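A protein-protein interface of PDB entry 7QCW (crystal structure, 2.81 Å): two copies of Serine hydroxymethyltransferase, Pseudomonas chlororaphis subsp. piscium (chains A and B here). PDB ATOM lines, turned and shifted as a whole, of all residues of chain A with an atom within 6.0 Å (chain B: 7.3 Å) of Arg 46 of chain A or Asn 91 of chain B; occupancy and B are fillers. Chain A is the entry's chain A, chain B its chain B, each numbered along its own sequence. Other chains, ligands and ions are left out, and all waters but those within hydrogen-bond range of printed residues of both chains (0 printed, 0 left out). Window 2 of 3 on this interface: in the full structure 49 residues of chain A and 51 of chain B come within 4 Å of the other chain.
OE2 of Glu 43 of chain A sits close to OD1 of Asn 91 of chain B (3.3 Å). O of Ala 71 of chain B is in hydrogen-bond range of NE2 of Gln 47 of chain A (2.6 Å). ND2 of Asn 74 of chain B sits at hydrogen-bond distance from OE1 of Gln 47 of chain A (2.9 Å).
The side-chain carboxylate (OE1) of Glu 43 of chain A lies within salt-bridge range of the guanidinium group (NH2) of Arg 46 of chain A, at 2.8 Å. OE1 of Glu 43 of chain A is in hydrogen-bond range of NE2 of Gln 47 of chain A (3.1 Å). OG1 of Thr 50 of chain A sits at hydrogen-bond distance from O of Arg 46 of chain A (2.8 Å). The backbone carbonyl oxygen (O) of Gln 47 of chain A lies within hydrogen-bond range of the guanidinium group (NH2) of Arg 400 of chain A (3.2 Å). O of Ala 71 of chain B sits at hydrogen-bond distance from ND2 of Asn 74 of chain B, at 3.1 Å.
Among the printed residues, pairs that only touch across the chains: Ile 39 of chain A with Asn 91 of chain B (3.7 Å), Ile 39 of chain A with Val 95 of chain B (3.4 Å), Ala 42 of chain A with Asn 91 of chain B (3.9 Å), Glu 43 of chain A with Leu 72 of chain B (3.4 Å), Glu 43 of chain A with Val 75 of chain B (3.2 Å), Arg 46 of chain A with Gly 88 of chain B (3.5 Å), Arg 46 of chain A with Asn 91 of chain B (3.8 Å) and Gln 47 of chain A with Val 75 of chain B (3.6 Å).
Of chain B, only Gly 88 (3.5 Å) and Asn 91 (3.8 Å) come within 4 Å of Arg 46 of chain A. Of chain A, only Ile 39, Ala 42, Glu 43 and Arg 46 come within 4 Å of Asn 91 of chain B. Printed residues of chain A within 4 Å of Val 95 of chain B: Ile 39. Printed residues of chain B within 4 Å of Ala 42 of chain A: Asn 91 (3.9 Å). Of the printed residues of chain A, Leu 72 of chain B touches Glu 43 (3.4 Å). Printed residues of chain A within 4 Å of Ala 71 of chain B: Gln 47 (2.6 Å). The nearest residue of chain A that does not touch Asn 91 of chain B is Arg 49 of chain A (5.6 Å). The nearest printed residue of chain B that does not touch Glu 43 of chain A is Gly 88 of chain B (4.4 Å).
Of the 12 printed residues of chain A, 5 touch a printed residue of chain B. Hydrophobic or aromatic side chains of chain A within 4 Å of the printed part of chain B: Ile 39. Of the 16 printed residues of chain B, 7 touch a printed residue of chain A. Hydrophobic or aromatic side chains of chain B that line the printed part of chain A: Ala 71, Leu 72, Val 75 and Val 95. Among the printed residues, 11 pairs touch across the chains.
No position is printed for both chains.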
ATOM      1  N   ILE A  39      19.659  27.160 -15.719  1.00  0.00           N
ATOM      2  CA  ILE A  39      20.965  26.590 -16.050  1.00  0.00           C
ATOM      3  C   ILE A  39      20.831  25.510 -17.118  1.00  0.00           C
ATOM      4  O   ILE A  39      21.680  25.386 -18.010  1.00  0.00           O
ATOM      5  CB  ILE A  39      21.663  26.048 -14.786  1.00  0.00           C
ATOM      6  CG1 ILE A  39      22.001  27.173 -13.798  1.00  0.00           C
ATOM      7  CG2 ILE A  39      22.930  25.337 -15.169  1.00  0.00           C
ATOM      8  CD1 ILE A  39      20.958  27.473 -12.760  1.00  0.00           C
ATOM      9  N   ASP A  41      18.581  25.361 -19.500  1.00  0.00           N
ATOM     10  CA  ASP A  41      18.376  26.048 -20.768  1.00  0.00           C
ATOM     11  C   ASP A  41      19.629  26.789 -21.215  1.00  0.00           C
ATOM     12  O   ASP A  41      19.888  26.898 -22.419  1.00  0.00           O
ATOM     13  CB  ASP A  41      17.199  27.017 -20.650  1.00  0.00           C
ATOM     14  CG  ASP A  41      15.858  26.327 -20.805  1.00  0.00           C
ATOM     15  OD1 ASP A  41      15.838  25.147 -21.212  1.00  0.00           O
ATOM     16  OD2 ASP A  41      14.824  26.964 -20.513  1.00  0.00           O
ATOM     17  N   ALA A  42      20.413  27.307 -20.265  1.00  0.00           N
ATOM     18  CA  ALA A  42      21.601  28.078 -20.618  1.00  0.00           C
ATOM     19  C   ALA A  42      22.674  27.197 -21.248  1.00  0.00           C
ATOM     20  O   ALA A  42      23.390  27.639 -22.154  1.00  0.00           O
ATOM     21  CB  ALA A  42      22.150  28.792 -19.384  1.00  0.00           C
ATOM     22  N   GLU A  43      22.813  25.957 -20.773  1.00  0.00           N
ATOM     23  CA  GLU A  43      23.829  25.072 -21.333  1.00  0.00           C
ATOM     24  C   GLU A  43      23.529  24.722 -22.784  1.00  0.00           C
ATOM     25  O   GLU A  43      24.437  24.716 -23.625  1.00  0.00           O
ATOM     26  CB  GLU A  43      23.949  23.797 -20.503  1.00  0.00           C
ATOM     27  CG  GLU A  43      24.975  22.833 -21.070  1.00  0.00           C
ATOM     28  CD  GLU A  43      26.396  23.329 -20.891  1.00  0.00           C
ATOM     29  OE1 GLU A  43      27.257  23.005 -21.734  1.00  0.00           O
ATOM     30  OE2 GLU A  43      26.659  24.040 -19.903  1.00  0.00           O
ATOM     31  N   VAL A  44      22.267  24.414 -23.094  1.00  0.00           N
ATOM     32  CA  VAL A  44      21.887  24.109 -24.472  1.00  0.00           C
ATOM     33  C   VAL A  44      22.265  25.267 -25.387  1.00  0.00           C
ATOM     34  O   VAL A  44      22.828  25.072 -26.470  1.00  0.00           O
ATOM     35  CB  VAL A  44      20.383  23.791 -24.558  1.00  0.00           C
ATOM     36  CG1 VAL A  44      20.015  23.343 -25.965  1.00  0.00           C
ATOM     37  CG2 VAL A  44      20.007  22.727 -23.541  1.00  0.00           C
ATOM     38  N   ALA A  45      21.963  26.493 -24.955  1.00  0.00           N
ATOM     39  CA  ALA A  45      22.363  27.671 -25.718  1.00  0.00           C
ATOM     40  C   ALA A  45      23.881  27.766 -25.827  1.00  0.00           C
ATOM     41  O   ALA A  45      24.423  28.011 -26.911  1.00  0.00           O
ATOM     42  CB  ALA A  45      21.787  28.931 -25.072  1.00  0.00           C
ATOM     43  N   ARG A  46      24.583  27.562 -24.708  1.00  0.00           N
ATOM     44  CA  ARG A  46      26.041  27.655 -24.715  1.00  0.00           C
ATOM     45  C   ARG A  46      26.668  26.644 -25.671  1.00  0.00           C
ATOM     46  O   ARG A  46      27.602  26.979 -26.409  1.00  0.00           O
ATOM     47  CB  ARG A  46      26.584  27.467 -23.296  1.00  0.00           C
ATOM     48  CG  ARG A  46      28.059  27.793 -23.152  1.00  0.00           C
ATOM     49  CD  ARG A  46      28.646  27.151 -21.899  1.00  0.00           C
ATOM     50  NE  ARG A  46      28.825  25.701 -22.019  1.00  0.00           N
ATOM     51  CZ  ARG A  46      29.572  25.087 -22.937  1.00  0.00           C
ATOM     52  NH1 ARG A  46      30.259  25.778 -23.838  1.00  0.00           N
ATOM     53  NH2 ARG A  46      29.649  23.762 -22.937  1.00  0.00           N
ATOM     54  N   GLN A  47      26.171  25.399 -25.667  1.00  0.00           N
ATOM     55  CA  GLN A  47      26.696  24.352 -26.542  1.00  0.00           C
ATOM     56  C   GLN A  47      26.475  24.650 -28.009  1.00  0.00           C
ATOM     57  O   GLN A  47      27.174  24.085 -28.852  1.00  0.00           O
ATOM     58  CB  GLN A  47      26.062  23.002 -26.177  1.00  0.00           C
ATOM     59  CG  GLN A  47      26.395  22.512 -24.812  1.00  0.00           C
ATOM     60  CD  GLN A  47      25.861  21.128 -24.567  1.00  0.00           C
ATOM     61  OE1 GLN A  47      25.289  20.500 -25.458  1.00  0.00           O
ATOM     62  NE2 GLN A  47      26.041  20.640 -23.349  1.00  0.00           N
ATOM     63  N   GLN A  48      25.499  25.487 -28.308  1.00  0.00           N
ATOM     64  CA  GLN A  48      25.108  25.928 -29.641  1.00  0.00           C
ATOM     65  C   GLN A  48      25.660  27.278 -30.042  1.00  0.00           C
ATOM     66  O   GLN A  48      25.750  27.548 -31.246  1.00  0.00           O
ATOM     67  CB  GLN A  48      23.584  25.958 -29.740  1.00  0.00           C
ATOM     68  CG  GLN A  48      22.853  26.634 -30.911  1.00  0.00           C
ATOM     69  CD  GLN A  48      23.322  26.224 -32.340  1.00  0.00           C
ATOM     70  OE1 GLN A  48      23.873  27.034 -33.066  1.00  0.00           O
ATOM     71  NE2 GLN A  48      23.162  24.912 -32.693  1.00  0.00           N
ATOM     72  N   ARG A  49      26.075  28.109 -29.087  1.00  0.00           N
ATOM     73  CA  ARG A  49      26.833  29.302 -29.423  1.00  0.00           C
ATOM     74  C   ARG A  49      28.336  29.058 -29.417  1.00  0.00           C
ATOM     75  O   ARG A  49      29.099  29.994 -29.662  1.00  0.00           O
ATOM     76  CB  ARG A  49      26.469  30.438 -28.467  1.00  0.00           C
ATOM     77  CG  ARG A  49      27.317  30.506 -27.191  1.00  0.00           C
ATOM     78  CD  ARG A  49      26.949  31.703 -26.320  1.00  0.00           C
ATOM     79  NE  ARG A  49      27.470  31.582 -24.959  1.00  0.00           N
ATOM     80  CZ  ARG A  49      26.705  31.516 -23.872  1.00  0.00           C
ATOM     81  NH1 ARG A  49      25.384  31.551 -23.985  1.00  0.00           N
ATOM     82  NH2 ARG A  49      27.259  31.407 -22.673  1.00  0.00           N
ATOM     83  N   THR A  50      28.773  27.829 -29.150  1.00  0.00           N
ATOM     84  CA  THR A  50      30.189  27.491 -29.063  1.00  0.00           C
ATOM     85  C   THR A  50      30.584  26.578 -30.218  1.00  0.00           C
ATOM     86  O   THR A  50      29.911  25.576 -30.483  1.00  0.00           O
ATOM     87  CB  THR A  50      30.511  26.815 -27.725  1.00  0.00           C
ATOM     88  OG1 THR A  50      30.277  27.730 -26.646  1.00  0.00           O
ATOM     89  CG2 THR A  50      31.970  26.350 -27.685  1.00  0.00           C
ATOM     90  N   ARG A 400      26.539  19.713 -37.117  1.00  0.00           N
ATOM     91  CA  ARG A 400      26.174  21.061 -37.521  1.00  0.00           C
ATOM     92  C   ARG A 400      25.941  21.175 -39.021  1.00  0.00           C
ATOM     93  O   ARG A 400      25.625  22.268 -39.502  1.00  0.00           O
ATOM     94  CB  ARG A 400      27.261  22.047 -37.083  1.00  0.00           C
ATOM     95  CG  ARG A 400      27.250  22.346 -35.592  1.00  0.00           C
ATOM     96  CD  ARG A 400      28.170  23.504 -35.256  1.00  0.00           C
ATOM     97  NE  ARG A 400      28.217  23.770 -33.821  1.00  0.00           N
ATOM     98  CZ  ARG A 400      27.453  24.665 -33.204  1.00  0.00           C
ATOM     99  NH1 ARG A 400      26.581  25.383 -33.898  1.00  0.00           N
ATOM    100  NH2 ARG A 400      27.560  24.845 -31.895  1.00  0.00           N
ATOM    101  N   ALA B  71      21.340  18.294 -21.551  1.00  0.00           N
ATOM    102  CA  ALA B  71      22.427  18.291 -22.521  1.00  0.00           C
ATOM    103  C   ALA B  71      23.784  18.502 -21.866  1.00  0.00           C
ATOM    104  O   ALA B  71      24.804  18.502 -22.563  1.00  0.00           O
ATOM    105  CB  ALA B  71      22.192  19.362 -23.590  1.00  0.00           C
ATOM    106  N   LEU B  72      23.811  18.678 -20.543  1.00  0.00           N
ATOM    107  CA  LEU B  72      25.061  18.691 -19.795  1.00  0.00           C
ATOM    108  C   LEU B  72      25.783  17.353 -19.879  1.00  0.00           C
ATOM    109  O   LEU B  72      26.968  17.272 -19.532  1.00  0.00           O
ATOM    110  CB  LEU B  72      24.770  19.064 -18.343  1.00  0.00           C
ATOM    111  CG  LEU B  72      24.549  20.551 -18.068  1.00  0.00           C
ATOM    112  CD1 LEU B  72      23.981  20.785 -16.687  1.00  0.00           C
ATOM    113  CD2 LEU B  72      25.867  21.265 -18.183  1.00  0.00           C
ATOM    114  N   ASN B  74      26.623  16.194 -22.598  1.00  0.00           N
ATOM    115  CA  ASN B  74      27.591  16.459 -23.656  1.00  0.00           C
ATOM    116  C   ASN B  74      28.842  17.172 -23.159  1.00  0.00           C
ATOM    117  O   ASN B  74      29.791  17.330 -23.934  1.00  0.00           O
ATOM    118  CB  ASN B  74      26.940  17.280 -24.772  1.00  0.00           C
ATOM    119  CG  ASN B  74      25.581  16.744 -25.174  1.00  0.00           C
ATOM    120  OD1 ASN B  74      25.366  15.532 -25.204  1.00  0.00           O
ATOM    121  ND2 ASN B  74      24.663  17.643 -25.507  1.00  0.00           N
ATOM    122  N   VAL B  75      28.865  17.614 -21.905  1.00  0.00           N
ATOM    123  CA  VAL B  75      30.049  18.233 -21.323  1.00  0.00           C
ATOM    124  C   VAL B  75      30.909  17.147 -20.694  1.00  0.00           C
ATOM    125  O   VAL B  75      30.432  16.367 -19.861  1.00  0.00           O
ATOM    126  CB  VAL B  75      29.666  19.299 -20.285  1.00  0.00           C
ATOM    127  CG1 VAL B  75      30.904  20.048 -19.820  1.00  0.00           C
ATOM    128  CG2 VAL B  75      28.640  20.256 -20.865  1.00  0.00           C
ATOM    129  N   ALA B  87      35.322  29.245 -20.506  1.00  0.00           N
ATOM    130  CA  ALA B  87      35.042  28.038 -19.738  1.00  0.00           C
ATOM    131  C   ALA B  87      33.759  27.365 -20.212  1.00  0.00           C
ATOM    132  O   ALA B  87      32.695  27.985 -20.247  1.00  0.00           O
ATOM    133  CB  ALA B  87      34.949  28.365 -18.252  1.00  0.00           C
ATOM    134  N   GLY B  88      33.873  26.098 -20.598  1.00  0.00           N
ATOM    135  CA  GLY B  88      32.721  25.271 -20.873  1.00  0.00           C
ATOM    136  C   GLY B  88      32.179  24.548 -19.664  1.00  0.00           C
ATOM    137  O   GLY B  88      31.158  23.864 -19.774  1.00  0.00           O
ATOM    138  N   CYS B  89      32.844  24.674 -18.511  1.00  0.00           N
ATOM    139  CA  CYS B  89      32.465  24.015 -17.264  1.00  0.00           C
ATOM    140  C   CYS B  89      31.760  24.946 -16.287  1.00  0.00           C
ATOM    141  O   CYS B  89      31.444  24.544 -15.174  1.00  0.00           O
ATOM    142  CB  CYS B  89      33.695  23.397 -16.586  1.00  0.00           C
ATOM    143  SG  CYS B  89      34.120  21.733 -17.144  1.00  0.00           S
ATOM    144  N   GLU B  90      31.540  26.194 -16.663  1.00  0.00           N
ATOM    145  CA  GLU B  90      30.764  27.088 -15.813  1.00  0.00           C
ATOM    146  C   GLU B  90      29.359  26.563 -15.525  1.00  0.00           C
ATOM    147  O   GLU B  90      29.019  26.358 -14.357  1.00  0.00           O
ATOM    148  CB  GLU B  90      30.863  28.515 -16.377  1.00  0.00           C
ATOM    149  CG  GLU B  90      29.766  29.607 -16.217  1.00  0.00           C
ATOM    150  CD  GLU B  90      30.430  30.970 -16.315  1.00  0.00           C
ATOM    151  OE1 GLU B  90      31.613  31.008 -15.952  1.00  0.00           O
ATOM    152  OE2 GLU B  90      29.824  31.850 -17.020  1.00  0.00           O
ATOM    153  N   ASN B  91      28.538  26.272 -16.536  1.00  0.00           N
ATOM    154  CA  ASN B  91      27.193  25.805 -16.179  1.00  0.00           C
ATOM    155  C   ASN B  91      27.226  24.491 -15.394  1.00  0.00           C
ATOM    156  O   ASN B  91      26.366  24.275 -14.532  1.00  0.00           O
ATOM    157  CB  ASN B  91      26.292  25.669 -17.405  1.00  0.00           C
ATOM    158  CG  ASN B  91      25.902  27.006 -17.984  1.00  0.00           C
ATOM    159  OD1 ASN B  91      25.963  27.206 -19.197  1.00  0.00           O
ATOM    160  ND2 ASN B  91      25.512  27.939 -17.122  1.00  0.00           N
ATOM    161  N   VAL B  92      28.206  23.614 -15.648  1.00  0.00           N
ATOM    162  CA  VAL B  92      28.304  22.398 -14.837  1.00  0.00           C
ATOM    163  C   VAL B  92      28.683  22.771 -13.411  1.00  0.00           C
ATOM    164  O   VAL B  92      28.244  22.136 -12.444  1.00  0.00           O
ATOM    165  CB  VAL B  92      29.310  21.383 -15.432  1.00  0.00           C
ATOM    166  CG1 VAL B  92      29.021  21.090 -16.891  1.00  0.00           C
ATOM    167  CG2 VAL B  92      30.761  21.732 -15.173  1.00  0.00           C
ATOM    168  N   ASP B  93      29.519  23.805 -13.260  1.00  0.00           N
ATOM    169  CA  ASP B  93      29.828  24.337 -11.940  1.00  0.00           C
ATOM    170  C   ASP B  93      28.592  24.951 -11.299  1.00  0.00           C
ATOM    171  O   ASP B  93      28.421  24.876 -10.078  1.00  0.00           O
ATOM    172  CB  ASP B  93      30.948  25.373 -12.039  1.00  0.00           C
ATOM    173  CG  ASP B  93      32.296  24.753 -12.357  1.00  0.00           C
ATOM    174  OD1 ASP B  93      32.417  23.509 -12.294  1.00  0.00           O
ATOM    175  OD2 ASP B  93      33.235  25.512 -12.679  1.00  0.00           O
ATOM    176  N   LEU B  94      27.724  25.582 -12.100  1.00  0.00           N
ATOM    177  CA  LEU B  94      26.529  26.176 -11.511  1.00  0.00           C
ATOM    178  C   LEU B  94      25.580  25.092 -11.007  1.00  0.00           C
ATOM    179  O   LEU B  94      25.008  25.217  -9.916  1.00  0.00           O
ATOM    180  CB  LEU B  94      25.797  27.093 -12.497  1.00  0.00           C
ATOM    181  CG  LEU B  94      26.284  28.521 -12.833  1.00  0.00           C
ATOM    182  CD1 LEU B  94      26.596  29.370 -11.580  1.00  0.00           C
ATOM    183  CD2 LEU B  94      27.301  28.683 -13.960  1.00  0.00           C
ATOM    184  N   VAL B  95      25.399  24.022 -11.789  1.00  0.00           N
ATOM    185  CA  VAL B  95      24.589  22.892 -11.337  1.00  0.00           C
ATOM    186  C   VAL B  95      25.195  22.274 -10.088  1.00  0.00           C
ATOM    187  O   VAL B  95      24.494  21.988  -9.108  1.00  0.00           O
ATOM    188  CB  VAL B  95      24.446  21.848 -12.457  1.00  0.00           C
ATOM    189  CG1 VAL B  95      23.897  20.545 -11.901  1.00  0.00           C
ATOM    190  CG2 VAL B  95      23.534  22.363 -13.529  1.00  0.00           C
ATOM    191  N   GLU B  96      26.511  22.058 -10.107  1.00  0.00           N
ATOM    192  CA  GLU B  96      27.159  21.414  -8.976  1.00  0.00           C
ATOM    193  C   GLU B  96      26.963  22.227  -7.707  1.00  0.00           C
ATOM    194  O   GLU B  96      26.523  21.691  -6.684  1.00  0.00           O
ATOM    195  CB  GLU B  96      28.645  21.209  -9.275  1.00  0.00           C
ATOM    196  CG  GLU B  96      29.381  20.437  -8.199  1.00  0.00           C
ATOM    197  CD  GLU B  96      30.633  19.757  -8.714  1.00  0.00           C
ATOM    198  OE1 GLU B  96      30.945  19.888  -9.919  1.00  0.00           O
ATOM    199  OE2 GLU B  96      31.308  19.089  -7.905  1.00  0.00           O
ATOM    200  N   SER B  97      27.201  23.538  -7.783  1.00  0.00           N
ATOM    201  CA  SER B  97      27.078  24.393  -6.609  1.00  0.00           C
ATOM    202  C   SER B  97      25.654  24.391  -6.062  1.00  0.00           C
ATOM    203  O   SER B  97      25.454  24.409  -4.841  1.00  0.00           O
ATOM    204  CB  SER B  97      27.519  25.815  -6.954  1.00  0.00           C
ATOM    205  OG  SER B  97      28.880  25.842  -7.351  1.00  0.00           O
ATOM    206  N   VAL B 295      27.158  14.908 -15.687  1.00  0.00           N
ATOM    207  CA  VAL B 295      26.528  16.084 -15.103  1.00  0.00           C
ATOM    208  C   VAL B 295      25.010  16.052 -15.276  1.00  0.00           C
ATOM    209  O   VAL B 295      24.295  16.744 -14.534  1.00  0.00           O
ATOM    210  CB  VAL B 295      27.186  17.351 -15.692  1.00  0.00           C
ATOM    211  CG1 VAL B 295      26.381  18.614 -15.391  1.00  0.00           C
ATOM    212  CG2 VAL B 295      28.619  17.479 -15.181  1.00  0.00           C
